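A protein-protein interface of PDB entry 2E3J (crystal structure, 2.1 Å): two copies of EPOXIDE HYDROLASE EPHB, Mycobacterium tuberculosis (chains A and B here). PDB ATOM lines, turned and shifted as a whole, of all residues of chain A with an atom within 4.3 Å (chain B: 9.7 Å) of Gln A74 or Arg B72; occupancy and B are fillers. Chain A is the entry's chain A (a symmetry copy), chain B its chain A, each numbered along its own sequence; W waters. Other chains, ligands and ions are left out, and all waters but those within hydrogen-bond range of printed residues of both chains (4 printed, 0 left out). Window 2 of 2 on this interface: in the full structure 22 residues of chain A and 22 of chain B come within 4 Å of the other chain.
Arg A72 touches its own counterpart, Arg B72.
Arg A72 touches Gln B171, and with the chains exchanged Gln A171 touches Arg B72.
Arg A72 touches Ile B175, and with the chains exchanged Ile A175 touches Arg B72.
Val A73 touches Gln B171, and with the chains exchanged Gln A171 touches Val B73.
The guanidinium group (NH2) of Arg A72 lies within hydrogen-bond range of the backbone carbonyl oxygen (O) of Arg B72 (2.7 Å).
NE2 of Gln A74 lies close to NH2 of Arg B72 (3.2 Å).
The guanidinium group (NE) of Arg B72 lies close to the side-chain amide nitrogen (NE2) of Gln A171.
The side-chain amide nitrogen (NE2) of Gln B74 sits close to the guanidinium group (NH2) of Arg A72 (3.2 Å).
The guanidinium group (NE) of Arg A72 sits close to the side-chain amide nitrogen (NE2) of Gln B171 (3.5 Å).
NZ of Lys A75 lies within salt-bridge range of OD1 of Asp B172.
CB of Arg A72 touches CD1 of Ile B175 (3.95 Å).
Gln B171 touches Val A73 (O to CG1, 3.7 Å).
Val A73 touches Asp B172.
Val B73 touches Gln A171.
CG2 of Ile A175 touches O of Lys B70, at 3.7 Å.
Ile A175 touches Arg B72 (CD1 to CB, 3.95 Å).
Water W3 lies within hydrogen-bond range of the side-chain hydroxyl of Ser B270 (2.8 Å), the backbone carbonyl oxygen of Arg B72 (2.8 Å) and the guanidinium group of Arg A72 (2.8 Å).
Water W1 lies within hydrogen-bond range of OG of Ser A270, O of Arg A72 and NE of Arg B72.
Water W4 lies within hydrogen-bond range of N of Arg B72 (2.8 Å), N of Val B73 (2.9 Å) and O of Gln A171 (3.0 Å).
Water W2 lies within hydrogen-bond range of N of Arg A72 (2.8 Å), N of Val A73 (2.9 Å) and O of Gln B171 (3.0 Å).
The side-chain amide oxygen (OE1) of Gln B74 lies within hydrogen-bond range of the side-chain hydroxyl (OG) of Ser B270 (2.8 Å).
O of Gln B74 lies within hydrogen-bond range of ND2 of Asn B274 (2.9 Å).
NE2 of Gln B171 sits at hydrogen-bond distance from O of Gly B266 (2.9 Å).
OG of Ser B270 lies within hydrogen-bond range of NE2 of Gln B171, 2.9 Å away.
The side-chain amide oxygen (OE1) of Gln A74 is in hydrogen-bond range of the side-chain hydroxyl (OG) of Ser A270, 2.8 Å away.
ND2 of Asn A274 is in hydrogen-bond range of O of Gln A74 (2.9 Å).
Among the printed residues, 12 pairs touch across the chains.
Among the printed residues, Asp or Glu carboxylates within 4 Å of a Lys or Arg side-chain nitrogen of the other chain: Lys A75 with Asp B172.
Gln A74 touches just one residue of chain B: Arg B72.
Of chain A, only Arg A72, Gln A74, Gln A171 and Ile A175 come within 4 Å of Arg B72.
No residue of chain B comes within 4 Å of Ser A270.
Printed residues of chain B within 4 Å of Lys A75: Asp B172 (3.6 Å).
Printed residues of chain A within 4 Å of Val B73: Gln A171 (3.7 Å).
The nearest residue of chain B that does not touch Gln A74 is Gln B171 (7.5 Å).
The nearest residue of chain A that does not touch Arg B72 is Ser A270 (4.2 Å).
The nearest printed residue of chain A that does not touch Asp B172 is Arg A72 (6.3 Å).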
ATOM      1  N   ARG A  72      23.705  -5.142  26.448  1.00  0.00           N
ATOM      2  CA  ARG A  72      23.389  -5.030  25.037  1.00  0.00           C
ATOM      3  C   ARG A  72      23.007  -6.395  24.474  1.00  0.00           C
ATOM      4  O   ARG A  72      22.069  -6.491  23.680  1.00  0.00           O
ATOM      5  CB  ARG A  72      24.562  -4.453  24.249  1.00  0.00           C
ATOM      6  CG  ARG A  72      24.174  -4.144  22.806  1.00  0.00           C
ATOM      7  CD  ARG A  72      25.277  -3.416  22.044  1.00  0.00           C
ATOM      8  NE  ARG A  72      24.795  -2.992  20.728  1.00  0.00           N
ATOM      9  CZ  ARG A  72      24.464  -3.836  19.754  1.00  0.00           C
ATOM     10  NH1 ARG A  72      24.573  -5.143  19.946  1.00  0.00           N
ATOM     11  NH2 ARG A  72      24.008  -3.375  18.596  1.00  0.00           N
ATOM     12  N   VAL A  73      23.717  -7.448  24.882  1.00  0.00           N
ATOM     13  CA  VAL A  73      23.408  -8.792  24.382  1.00  0.00           C
ATOM     14  C   VAL A  73      21.981  -9.165  24.730  1.00  0.00           C
ATOM     15  O   VAL A  73      21.476  -8.820  25.803  1.00  0.00           O
ATOM     16  CB  VAL A  73      24.355  -9.880  24.961  1.00  0.00           C
ATOM     17  CG1 VAL A  73      25.807  -9.555  24.602  1.00  0.00           C
ATOM     18  CG2 VAL A  73      24.160 -10.005  26.472  1.00  0.00           C
ATOM     19  N   GLN A  74      21.335  -9.878  23.820  1.00  0.00           N
ATOM     20  CA  GLN A  74      19.948 -10.286  23.997  1.00  0.00           C
ATOM     21  C   GLN A  74      19.705 -11.268  25.136  1.00  0.00           C
ATOM     22  O   GLN A  74      18.693 -11.176  25.830  1.00  0.00           O
ATOM     23  CB  GLN A  74      19.421 -10.888  22.693  1.00  0.00           C
ATOM     24  CG  GLN A  74      19.492  -9.943  21.516  1.00  0.00           C
ATOM     25  CD  GLN A  74      18.519  -8.794  21.634  1.00  0.00           C
ATOM     26  OE1 GLN A  74      17.854  -8.624  22.662  1.00  0.00           O
ATOM     27  NE2 GLN A  74      18.428  -7.992  20.584  1.00  0.00           N
ATOM     28  N   LYS A  75      20.623 -12.207  25.337  1.00  0.00           N
ATOM     29  CA  LYS A  75      20.427 -13.199  26.389  1.00  0.00           C
ATOM     30  C   LYS A  75      20.337 -12.615  27.800  1.00  0.00           C
ATOM     31  O   LYS A  75      19.854 -13.277  28.725  1.00  0.00           O
ATOM     32  CB  LYS A  75      21.523 -14.267  26.335  1.00  0.00           C
ATOM     33  CG  LYS A  75      22.928 -13.750  26.528  1.00  0.00           C
ATOM     34  CD  LYS A  75      23.881 -14.899  26.873  1.00  0.00           C
ATOM     35  CE  LYS A  75      25.330 -14.454  26.847  1.00  0.00           C
ATOM     36  NZ  LYS A  75      25.724 -14.062  25.466  1.00  0.00           N
ATOM     37  N   ALA A  76      20.795 -11.379  27.972  1.00  0.00           N
ATOM     38  CA  ALA A  76      20.735 -10.748  29.285  1.00  0.00           C
ATOM     39  C   ALA A  76      19.297 -10.386  29.640  1.00  0.00           C
ATOM     40  O   ALA A  76      18.994 -10.140  30.800  1.00  0.00           O
ATOM     41  CB  ALA A  76      21.616  -9.499  29.315  1.00  0.00           C
ATOM     42  N   TYR A  77      18.413 -10.377  28.643  1.00  0.00           N
ATOM     43  CA  TYR A  77      17.003 -10.028  28.850  1.00  0.00           C
ATOM     44  C   TYR A  77      16.000 -11.181  28.734  1.00  0.00           C
ATOM     45  O   TYR A  77      14.849 -10.978  28.352  1.00  0.00           O
ATOM     46  CB  TYR A  77      16.616  -8.896  27.891  1.00  0.00           C
ATOM     47  CG  TYR A  77      17.418  -7.636  28.154  1.00  0.00           C
ATOM     48  CD1 TYR A  77      17.155  -6.836  29.275  1.00  0.00           C
ATOM     49  CD2 TYR A  77      18.500  -7.297  27.345  1.00  0.00           C
ATOM     50  CE1 TYR A  77      17.960  -5.734  29.580  1.00  0.00           C
ATOM     51  CE2 TYR A  77      19.306  -6.206  27.641  1.00  0.00           C
ATOM     52  CZ  TYR A  77      19.032  -5.426  28.759  1.00  0.00           C
ATOM     53  OH  TYR A  77      19.833  -4.339  29.035  1.00  0.00           O
ATOM     54  N   ARG A  78      16.442 -12.385  29.083  1.00  0.00           N
ATOM     55  CA  ARG A  78      15.582 -13.564  29.047  1.00  0.00           C
ATOM     56  C   ARG A  78      14.868 -13.653  30.391  1.00  0.00           C
ATOM     57  O   ARG A  78      15.424 -13.260  31.417  1.00  0.00           O
ATOM     58  CB  ARG A  78      16.420 -14.816  28.797  1.00  0.00           C
ATOM     59  CG  ARG A  78      17.369 -14.653  27.621  1.00  0.00           C
ATOM     60  CD  ARG A  78      17.935 -15.972  27.154  1.00  0.00           C
ATOM     61  NE  ARG A  78      16.952 -16.739  26.399  1.00  0.00           N
ATOM     62  CZ  ARG A  78      17.217 -17.894  25.796  1.00  0.00           C
ATOM     63  NH1 ARG A  78      16.269 -18.529  25.123  1.00  0.00           N
ATOM     64  NH2 ARG A  78      18.433 -18.418  25.871  1.00  0.00           N
ATOM     65  N   GLN A 171      13.968  -3.615  17.169  1.00  0.00           N
ATOM     66  CA  GLN A 171      14.843  -2.634  17.807  1.00  0.00           C
ATOM     67  C   GLN A 171      15.640  -1.767  16.837  1.00  0.00           C
ATOM     68  O   GLN A 171      16.804  -1.472  17.080  1.00  0.00           O
ATOM     69  CB  GLN A 171      15.808  -3.356  18.750  1.00  0.00           C
ATOM     70  CG  GLN A 171      15.134  -4.072  19.914  1.00  0.00           C
ATOM     71  CD  GLN A 171      16.098  -4.954  20.682  1.00  0.00           C
ATOM     72  OE1 GLN A 171      16.479  -6.034  20.217  1.00  0.00           O
ATOM     73  NE2 GLN A 171      16.513  -4.493  21.861  1.00  0.00           N
ATOM     74  N   ILE A 175      12.943   2.247  17.668  1.00  0.00           N
ATOM     75  CA  ILE A 175      13.780   3.196  18.383  1.00  0.00           C
ATOM     76  C   ILE A 175      13.913   4.495  17.588  1.00  0.00           C
ATOM     77  O   ILE A 175      13.862   5.590  18.154  1.00  0.00           O
ATOM     78  CB  ILE A 175      15.165   2.580  18.663  1.00  0.00           C
ATOM     79  CG1 ILE A 175      15.006   1.466  19.707  1.00  0.00           C
ATOM     80  CG2 ILE A 175      16.133   3.639  19.132  1.00  0.00           C
ATOM     81  CD1 ILE A 175      16.277   0.735  20.060  1.00  0.00           C
ATOM     82  N   SER A 270      14.411  -5.352  24.395  1.00  0.00           N
ATOM     83  CA  SER A 270      14.957  -6.698  24.323  1.00  0.00           C
ATOM     84  C   SER A 270      14.054  -7.692  25.055  1.00  0.00           C
ATOM     85  O   SER A 270      14.132  -8.895  24.821  1.00  0.00           O
ATOM     86  CB  SER A 270      16.366  -6.745  24.909  1.00  0.00           C
ATOM     87  OG  SER A 270      17.308  -6.263  23.969  1.00  0.00           O
ATOM     88  N   HIS A 273      11.827  -8.928  22.435  1.00  0.00           N
ATOM     89  CA  HIS A 273      12.644  -9.675  21.494  1.00  0.00           C
ATOM     90  C   HIS A 273      12.902 -11.109  21.947  1.00  0.00           C
ATOM     91  O   HIS A 273      13.085 -12.006  21.125  1.00  0.00           O
ATOM     92  CB  HIS A 273      13.968  -8.929  21.296  1.00  0.00           C
ATOM     93  CG  HIS A 273      14.904  -9.578  20.323  1.00  0.00           C
ATOM     94  ND1 HIS A 273      15.699 -10.655  20.656  1.00  0.00           N
ATOM     95  CD2 HIS A 273      15.200  -9.279  19.036  1.00  0.00           C
ATOM     96  CE1 HIS A 273      16.447 -10.987  19.619  1.00  0.00           C
ATOM     97  NE2 HIS A 273      16.162 -10.168  18.623  1.00  0.00           N
ATOM     98  N   ASN A 274      12.894 -11.322  23.258  1.00  0.00           N
ATOM     99  CA  ASN A 274      13.166 -12.637  23.819  1.00  0.00           C
ATOM    100  C   ASN A 274      11.937 -13.494  24.118  1.00  0.00           C
ATOM    101  O   ASN A 274      12.072 -14.595  24.646  1.00  0.00           O
ATOM    102  CB  ASN A 274      13.987 -12.482  25.099  1.00  0.00           C
ATOM    103  CG  ASN A 274      15.437 -12.165  24.826  1.00  0.00           C
ATOM    104  OD1 ASN A 274      16.180 -13.007  24.324  1.00  0.00           O
ATOM    105  ND2 ASN A 274      15.851 -10.945  25.155  1.00  0.00           N
ATOM    106  N   ARG B  63      25.749  11.132  20.735  1.00  0.00           N
ATOM    107  CA  ARG B  63      24.705  10.127  20.718  1.00  0.00           C
ATOM    108  C   ARG B  63      25.184   8.902  21.481  1.00  0.00           C
ATOM    109  O   ARG B  63      26.355   8.555  21.423  1.00  0.00           O
ATOM    110  CB  ARG B  63      24.326   9.764  19.283  1.00  0.00           C
ATOM    111  CG  ARG B  63      25.478   9.315  18.415  1.00  0.00           C
ATOM    112  CD  ARG B  63      24.941   8.823  17.071  1.00  0.00           C
ATOM    113  NE  ARG B  63      24.149   9.832  16.364  1.00  0.00           N
ATOM    114  CZ  ARG B  63      23.367   9.559  15.325  1.00  0.00           C
ATOM    115  NH1 ARG B  63      23.272   8.312  14.877  1.00  0.00           N
ATOM    116  NH2 ARG B  63      22.676  10.524  14.736  1.00  0.00           N
ATOM    117  N   GLY B  64      24.268   8.264  22.208  1.00  0.00           N
ATOM    118  CA  GLY B  64      24.612   7.091  22.997  1.00  0.00           C
ATOM    119  C   GLY B  64      25.081   7.455  24.398  1.00  0.00           C
ATOM    120  O   GLY B  64      25.240   6.590  25.260  1.00  0.00           O
ATOM    121  N   SER B  69      20.125  10.878  22.366  1.00  0.00           N
ATOM    122  CA  SER B  69      19.511   9.678  21.798  1.00  0.00           C
ATOM    123  C   SER B  69      20.377   8.437  21.923  1.00  0.00           C
ATOM    124  O   SER B  69      21.599   8.491  21.714  1.00  0.00           O
ATOM    125  CB  SER B  69      19.170   9.910  20.328  1.00  0.00           C
ATOM    126  OG  SER B  69      18.116  10.838  20.217  1.00  0.00           O
ATOM    127  N   LYS B  70      19.730   7.324  22.267  1.00  0.00           N
ATOM    128  CA  LYS B  70      20.413   6.037  22.446  1.00  0.00           C
ATOM    129  C   LYS B  70      19.932   5.032  21.400  1.00  0.00           C
ATOM    130  O   LYS B  70      18.807   4.545  21.466  1.00  0.00           O
ATOM    131  CB  LYS B  70      20.126   5.459  23.841  1.00  0.00           C
ATOM    132  CG  LYS B  70      20.405   6.395  25.016  1.00  0.00           C
ATOM    133  CD  LYS B  70      21.875   6.697  25.181  1.00  0.00           C
ATOM    134  CE  LYS B  70      22.153   7.386  26.518  1.00  0.00           C
ATOM    135  NZ  LYS B  70      21.237   8.518  26.767  1.00  0.00           N
ATOM    136  N   TYR B  71      20.789   4.710  20.446  1.00  0.00           N
ATOM    137  CA  TYR B  71      20.422   3.754  19.402  1.00  0.00           C
ATOM    138  C   TYR B  71      21.010   2.400  19.718  1.00  0.00           C
ATOM    139  O   TYR B  71      22.015   2.304  20.424  1.00  0.00           O
ATOM    140  CB  TYR B  71      20.966   4.218  18.053  1.00  0.00           C
ATOM    141  CG  TYR B  71      20.359   5.509  17.591  1.00  0.00           C
ATOM    142  CD1 TYR B  71      19.042   5.556  17.124  1.00  0.00           C
ATOM    143  CD2 TYR B  71      21.078   6.696  17.656  1.00  0.00           C
ATOM    144  CE1 TYR B  71      18.464   6.754  16.735  1.00  0.00           C
ATOM    145  CE2 TYR B  71      20.505   7.899  17.272  1.00  0.00           C
ATOM    146  CZ  TYR B  71      19.202   7.922  16.813  1.00  0.00           C
ATOM    147  OH  TYR B  71      18.635   9.119  16.441  1.00  0.00           O
ATOM    148  N   ARG B  72      20.395   1.348  19.194  1.00  0.00           N
ATOM    149  CA  ARG B  72      20.932   0.020  19.415  1.00  0.00           C
ATOM    150  C   ARG B  72      21.653  -0.471  18.164  1.00  0.00           C
ATOM    151  O   ARG B  72      22.719  -1.080  18.268  1.00  0.00           O
ATOM    152  CB  ARG B  72      19.834  -0.967  19.802  1.00  0.00           C
ATOM    153  CG  ARG B  72      20.411  -2.313  20.232  1.00  0.00           C
ATOM    154  CD  ARG B  72      19.348  -3.260  20.779  1.00  0.00           C
ATOM    155  NE  ARG B  72      19.972  -4.463  21.333  1.00  0.00           N
ATOM    156  CZ  ARG B  72      20.621  -5.364  20.601  1.00  0.00           C
ATOM    157  NH1 ARG B  72      20.722  -5.202  19.288  1.00  0.00           N
ATOM    158  NH2 ARG B  72      21.185  -6.417  21.180  1.00  0.00           N
ATOM    159  N   VAL B  73      21.086  -0.205  16.985  1.00  0.00           N
ATOM    160  CA  VAL B  73      21.721  -0.647  15.738  1.00  0.00           C
ATOM    161  C   VAL B  73      23.106  -0.046  15.614  1.00  0.00           C
ATOM    162  O   VAL B  73      23.339   1.103  16.002  1.00  0.00           O
ATOM    163  CB  VAL B  73      20.902  -0.257  14.477  1.00  0.00           C
ATOM    164  CG1 VAL B  73      19.504  -0.874  14.549  1.00  0.00           C
ATOM    165  CG2 VAL B  73      20.842   1.263  14.331  1.00  0.00           C
ATOM    166  N   GLN B  74      24.026  -0.826  15.064  1.00  0.00           N
ATOM    167  CA  GLN B  74      25.408  -0.400  14.905  1.00  0.00           C
ATOM    168  C   GLN B  74      25.619   0.760  13.939  1.00  0.00           C
ATOM    169  O   GLN B  74      26.456   1.627  14.184  1.00  0.00           O
ATOM    170  CB  GLN B  74      26.262  -1.588  14.458  1.00  0.00           C
ATOM    171  CG  GLN B  74      26.231  -2.753  15.420  1.00  0.00           C
ATOM    172  CD  GLN B  74      26.940  -2.452  16.720  1.00  0.00           C
ATOM    173  OE1 GLN B  74      27.367  -1.320  16.966  1.00  0.00           O
ATOM    174  NE2 GLN B  74      27.069  -3.465  17.564  1.00  0.00           N
ATOM    175  N   LYS B  75      24.868   0.784  12.844  1.00  0.00           N
ATOM    176  CA  LYS B  75      25.051   1.849  11.863  1.00  0.00           C
ATOM    177  C   LYS B  75      24.777   3.256  12.399  1.00  0.00           C
ATOM    178  O   LYS B  75      25.200   4.250  11.799  1.00  0.00           O
ATOM    179  CB  LYS B  75      24.197   1.589  10.618  1.00  0.00           C
ATOM    180  CG  LYS B  75      22.710   1.524  10.867  1.00  0.00           C
ATOM    181  CD  LYS B  75      21.937   1.682   9.554  1.00  0.00           C
ATOM    182  CE  LYS B  75      20.459   1.394   9.733  1.00  0.00           C
ATOM    183  NZ  LYS B  75      20.254  -0.034  10.101  1.00  0.00           N
ATOM    184  N   ALA B  76      24.077   3.347  13.525  1.00  0.00           N
ATOM    185  CA  ALA B  76      23.785   4.652  14.105  1.00  0.00           C
ATOM    186  C   ALA B  76      25.045   5.266  14.705  1.00  0.00           C
ATOM    187  O   ALA B  76      25.084   6.464  14.956  1.00  0.00           O
ATOM    188  CB  ALA B  76      22.698   4.526  15.174  1.00  0.00           C
ATOM    189  N   TYR B  77      26.075   4.448  14.911  1.00  0.00           N
ATOM    190  CA  TYR B  77      27.338   4.913  15.499  1.00  0.00           C
ATOM    191  C   TYR B  77      28.539   4.976  14.549  1.00  0.00           C
ATOM    192  O   TYR B  77      29.684   4.813  14.970  1.00  0.00           O
ATOM    193  CB  TYR B  77      27.676   4.046  16.718  1.00  0.00           C
ATOM    194  CG  TYR B  77      26.624   4.165  17.802  1.00  0.00           C
ATOM    195  CD1 TYR B  77      26.529   5.319  18.593  1.00  0.00           C
ATOM    196  CD2 TYR B  77      25.659   3.173  17.973  1.00  0.00           C
ATOM    197  CE1 TYR B  77      25.495   5.477  19.520  1.00  0.00           C
ATOM    198  CE2 TYR B  77      24.628   3.322  18.889  1.00  0.00           C
ATOM    199  CZ  TYR B  77      24.550   4.475  19.662  1.00  0.00           C
ATOM    200  OH  TYR B  77      23.527   4.605  20.577  1.00  0.00           O
ATOM    201  N   VAL B 170      33.147  -6.066  20.890  1.00  0.00           N
ATOM    202  CA  VAL B 170      32.342  -7.269  21.087  1.00  0.00           C
ATOM    203  C   VAL B 170      31.064  -6.911  21.858  1.00  0.00           C
ATOM    204  O   VAL B 170      29.994  -7.470  21.602  1.00  0.00           O
ATOM    205  CB  VAL B 170      33.143  -8.368  21.841  1.00  0.00           C
ATOM    206  CG1 VAL B 170      32.293  -9.627  21.992  1.00  0.00           C
ATOM    207  CG2 VAL B 170      34.420  -8.693  21.076  1.00  0.00           C
ATOM    208  N   GLN B 171      31.190  -5.981  22.799  1.00  0.00           N
ATOM    209  CA  GLN B 171      30.049  -5.508  23.582  1.00  0.00           C
ATOM    210  C   GLN B 171      29.294  -6.604  24.329  1.00  0.00           C
ATOM    211  O   GLN B 171      28.071  -6.577  24.401  1.00  0.00           O
ATOM    212  CB  GLN B 171      29.080  -4.762  22.663  1.00  0.00           C
ATOM    213  CG  GLN B 171      29.654  -3.498  22.034  1.00  0.00           C
ATOM    214  CD  GLN B 171      28.746  -2.924  20.965  1.00  0.00           C
ATOM    215  OE1 GLN B 171      28.661  -3.456  19.853  1.00  0.00           O
ATOM    216  NE2 GLN B 171      28.049  -1.839  21.298  1.00  0.00           N
ATOM    217  N   ASP B 172      30.024  -7.569  24.875  1.00  0.00           N
ATOM    218  CA  ASP B 172      29.414  -8.656  25.622  1.00  0.00           C
ATOM    219  C   ASP B 172      30.133  -8.792  26.951  1.00  0.00           C
ATOM    220  O   ASP B 172      29.587  -8.445  27.997  1.00  0.00           O
ATOM    221  CB  ASP B 172      29.511  -9.977  24.851  1.00  0.00           C
ATOM    222  CG  ASP B 172      28.876 -11.146  25.607  1.00  0.00           C
ATOM    223  OD1 ASP B 172      28.805 -12.259  25.041  1.00  0.00           O
ATOM    224  OD2 ASP B 172      28.450 -10.956  26.768  1.00  0.00           O
ATOM    225  N   ILE B 175      31.016  -5.270  28.726  1.00  0.00           N
ATOM    226  CA  ILE B 175      29.905  -4.717  29.482  1.00  0.00           C
ATOM    227  C   ILE B 175      29.681  -5.516  30.765  1.00  0.00           C
ATOM    228  O   ILE B 175      29.429  -4.944  31.829  1.00  0.00           O
ATOM    229  CB  ILE B 175      28.630  -4.698  28.616  1.00  0.00           C
ATOM    230  CG1 ILE B 175      28.800  -3.649  27.509  1.00  0.00           C
ATOM    231  CG2 ILE B 175      27.415  -4.409  29.465  1.00  0.00           C
ATOM    232  CD1 ILE B 175      27.642  -3.539  26.550  1.00  0.00           C
ATOM    233  N   PHE B 265      26.893   1.327  28.508  1.00  0.00           N
ATOM    234  CA  PHE B 265      28.032   1.517  27.622  1.00  0.00           C
ATOM    235  C   PHE B 265      27.768   1.028  26.208  1.00  0.00           C
ATOM    236  O   PHE B 265      28.631   1.133  25.351  1.00  0.00           O
ATOM    237  CB  PHE B 265      29.262   0.819  28.195  1.00  0.00           C
ATOM    238  CG  PHE B 265      29.820   1.494  29.422  1.00  0.00           C
ATOM    239  CD1 PHE B 265      30.983   2.240  29.351  1.00  0.00           C
ATOM    240  CD2 PHE B 265      29.175   1.384  30.647  1.00  0.00           C
ATOM    241  CE1 PHE B 265      31.500   2.872  30.485  1.00  0.00           C
ATOM    242  CE2 PHE B 265      29.682   2.008  31.781  1.00  0.00           C
ATOM    243  CZ  PHE B 265      30.847   2.753  31.698  1.00  0.00           C
ATOM    244  N   GLY B 266      26.566   0.512  25.971  1.00  0.00           N
ATOM    245  CA  GLY B 266      26.207   0.012  24.655  1.00  0.00           C
ATOM    246  C   GLY B 266      26.495   0.976  23.520  1.00  0.00           C
ATOM    247  O   GLY B 266      27.297   0.677  22.641  1.00  0.00           O
ATOM    248  N   GLY B 267      25.841   2.134  23.533  1.00  0.00           N
ATOM    249  CA  GLY B 267      26.052   3.126  22.490  1.00  0.00           C
ATOM    250  C   GLY B 267      27.509   3.532  22.385  1.00  0.00           C
ATOM    251  O   GLY B 267      28.073   3.549  21.292  1.00  0.00           O
ATOM    252  N   PRO B 268      28.144   3.889  23.514  1.00  0.00           N
ATOM    253  CA  PRO B 268      29.548   4.288  23.533  1.00  0.00           C
ATOM    254  C   PRO B 268      30.483   3.260  22.877  1.00  0.00           C
ATOM    255  O   PRO B 268      31.326   3.616  22.043  1.00  0.00           O
ATOM    256  CB  PRO B 268      29.831   4.444  25.021  1.00  0.00           C
ATOM    257  CG  PRO B 268      28.531   4.976  25.541  1.00  0.00           C
ATOM    258  CD  PRO B 268      27.517   4.113  24.832  1.00  0.00           C
ATOM    259  N   LEU B 269      30.345   1.994  23.270  1.00  0.00           N
ATOM    260  CA  LEU B 269      31.194   0.940  22.725  1.00  0.00           C
ATOM    261  C   LEU B 269      30.966   0.697  21.236  1.00  0.00           C
ATOM    262  O   LEU B 269      31.855   0.206  20.550  1.00  0.00           O
ATOM    263  CB  LEU B 269      31.002  -0.365  23.510  1.00  0.00           C
ATOM    264  CG  LEU B 269      31.559  -0.315  24.935  1.00  0.00           C
ATOM    265  CD1 LEU B 269      31.126  -1.523  25.734  1.00  0.00           C
ATOM    266  CD2 LEU B 269      33.076  -0.227  24.862  1.00  0.00           C
ATOM    267  N   SER B 270      29.784   1.032  20.732  1.00  0.00           N
ATOM    268  CA  SER B 270      29.517   0.855  19.314  1.00  0.00           C
ATOM    269  C   SER B 270      30.440   1.734  18.471  1.00  0.00           C
ATOM    270  O   SER B 270      30.627   1.483  17.283  1.00  0.00           O
ATOM    271  CB  SER B 270      28.059   1.173  18.993  1.00  0.00           C
ATOM    272  OG  SER B 270      27.228   0.078  19.334  1.00  0.00           O
ATOM    273  N   PHE B 271      31.004   2.774  19.080  1.00  0.00           N
ATOM    274  CA  PHE B 271      31.935   3.645  18.369  1.00  0.00           C
ATOM    275  C   PHE B 271      33.102   2.754  17.930  1.00  0.00           C
ATOM    276  O   PHE B 271      33.440   2.679  16.748  1.00  0.00           O
ATOM    277  CB  PHE B 271      32.479   4.750  19.290  1.00  0.00           C
ATOM    278  CG  PHE B 271      31.552   5.944  19.476  1.00  0.00           C
ATOM    279  CD1 PHE B 271      30.252   5.782  19.937  1.00  0.00           C
ATOM    280  CD2 PHE B 271      32.029   7.241  19.277  1.00  0.00           C
ATOM    281  CE1 PHE B 271      29.434   6.894  20.208  1.00  0.00           C
ATOM    282  CE2 PHE B 271      31.229   8.360  19.541  1.00  0.00           C
ATOM    283  CZ  PHE B 271      29.930   8.189  20.009  1.00  0.00           C
ATOM    284  N   HIS B 273      33.289  -0.439  17.756  1.00  0.00           N
ATOM    285  CA  HIS B 273      32.805  -1.519  16.911  1.00  0.00           C
ATOM    286  C   HIS B 273      32.737  -1.128  15.438  1.00  0.00           C
ATOM    287  O   HIS B 273      32.872  -1.974  14.555  1.00  0.00           O
ATOM    288  CB  HIS B 273      31.425  -1.951  17.415  1.00  0.00           C
ATOM    289  CG  HIS B 273      30.812  -3.083  16.647  1.00  0.00           C
ATOM    290  ND1 HIS B 273      30.182  -2.907  15.433  1.00  0.00           N
ATOM    291  CD2 HIS B 273      30.702  -4.401  16.938  1.00  0.00           C
ATOM    292  CE1 HIS B 273      29.706  -4.065  15.012  1.00  0.00           C
ATOM    293  NE2 HIS B 273      30.009  -4.988  15.908  1.00  0.00           N
ATOM    294  N   ASN B 274      32.549   0.161  15.180  1.00  0.00           N
ATOM    295  CA  ASN B 274      32.427   0.656  13.816  1.00  0.00           C
ATOM    296  C   ASN B 274      33.718   1.171  13.183  1.00  0.00           C
ATOM    297  O   ASN B 274      33.694   1.659  12.056  1.00  0.00           O
ATOM    298  CB  ASN B 274      31.375   1.765  13.772  1.00  0.00           C
ATOM    299  CG  ASN B 274      29.965   1.232  13.834  1.00  0.00           C
ATOM    300  OD1 ASN B 274      29.491   0.598  12.892  1.00  0.00           O
ATOM    301  ND2 ASN B 274      29.281   1.486  14.946  1.00  0.00           N
HETATM  302  O   HOH W   1      19.765  -5.014  24.038  1.00  0.00           O
HETATM  303  O   HOH W   2      26.008  -6.780  26.602  1.00  0.00           O
HETATM  304  O   HOH W   3      24.611  -0.298  20.119  1.00  0.00           O
HETATM  305  O   HOH W   4      18.441   1.069  17.165  1.00  0.00           O
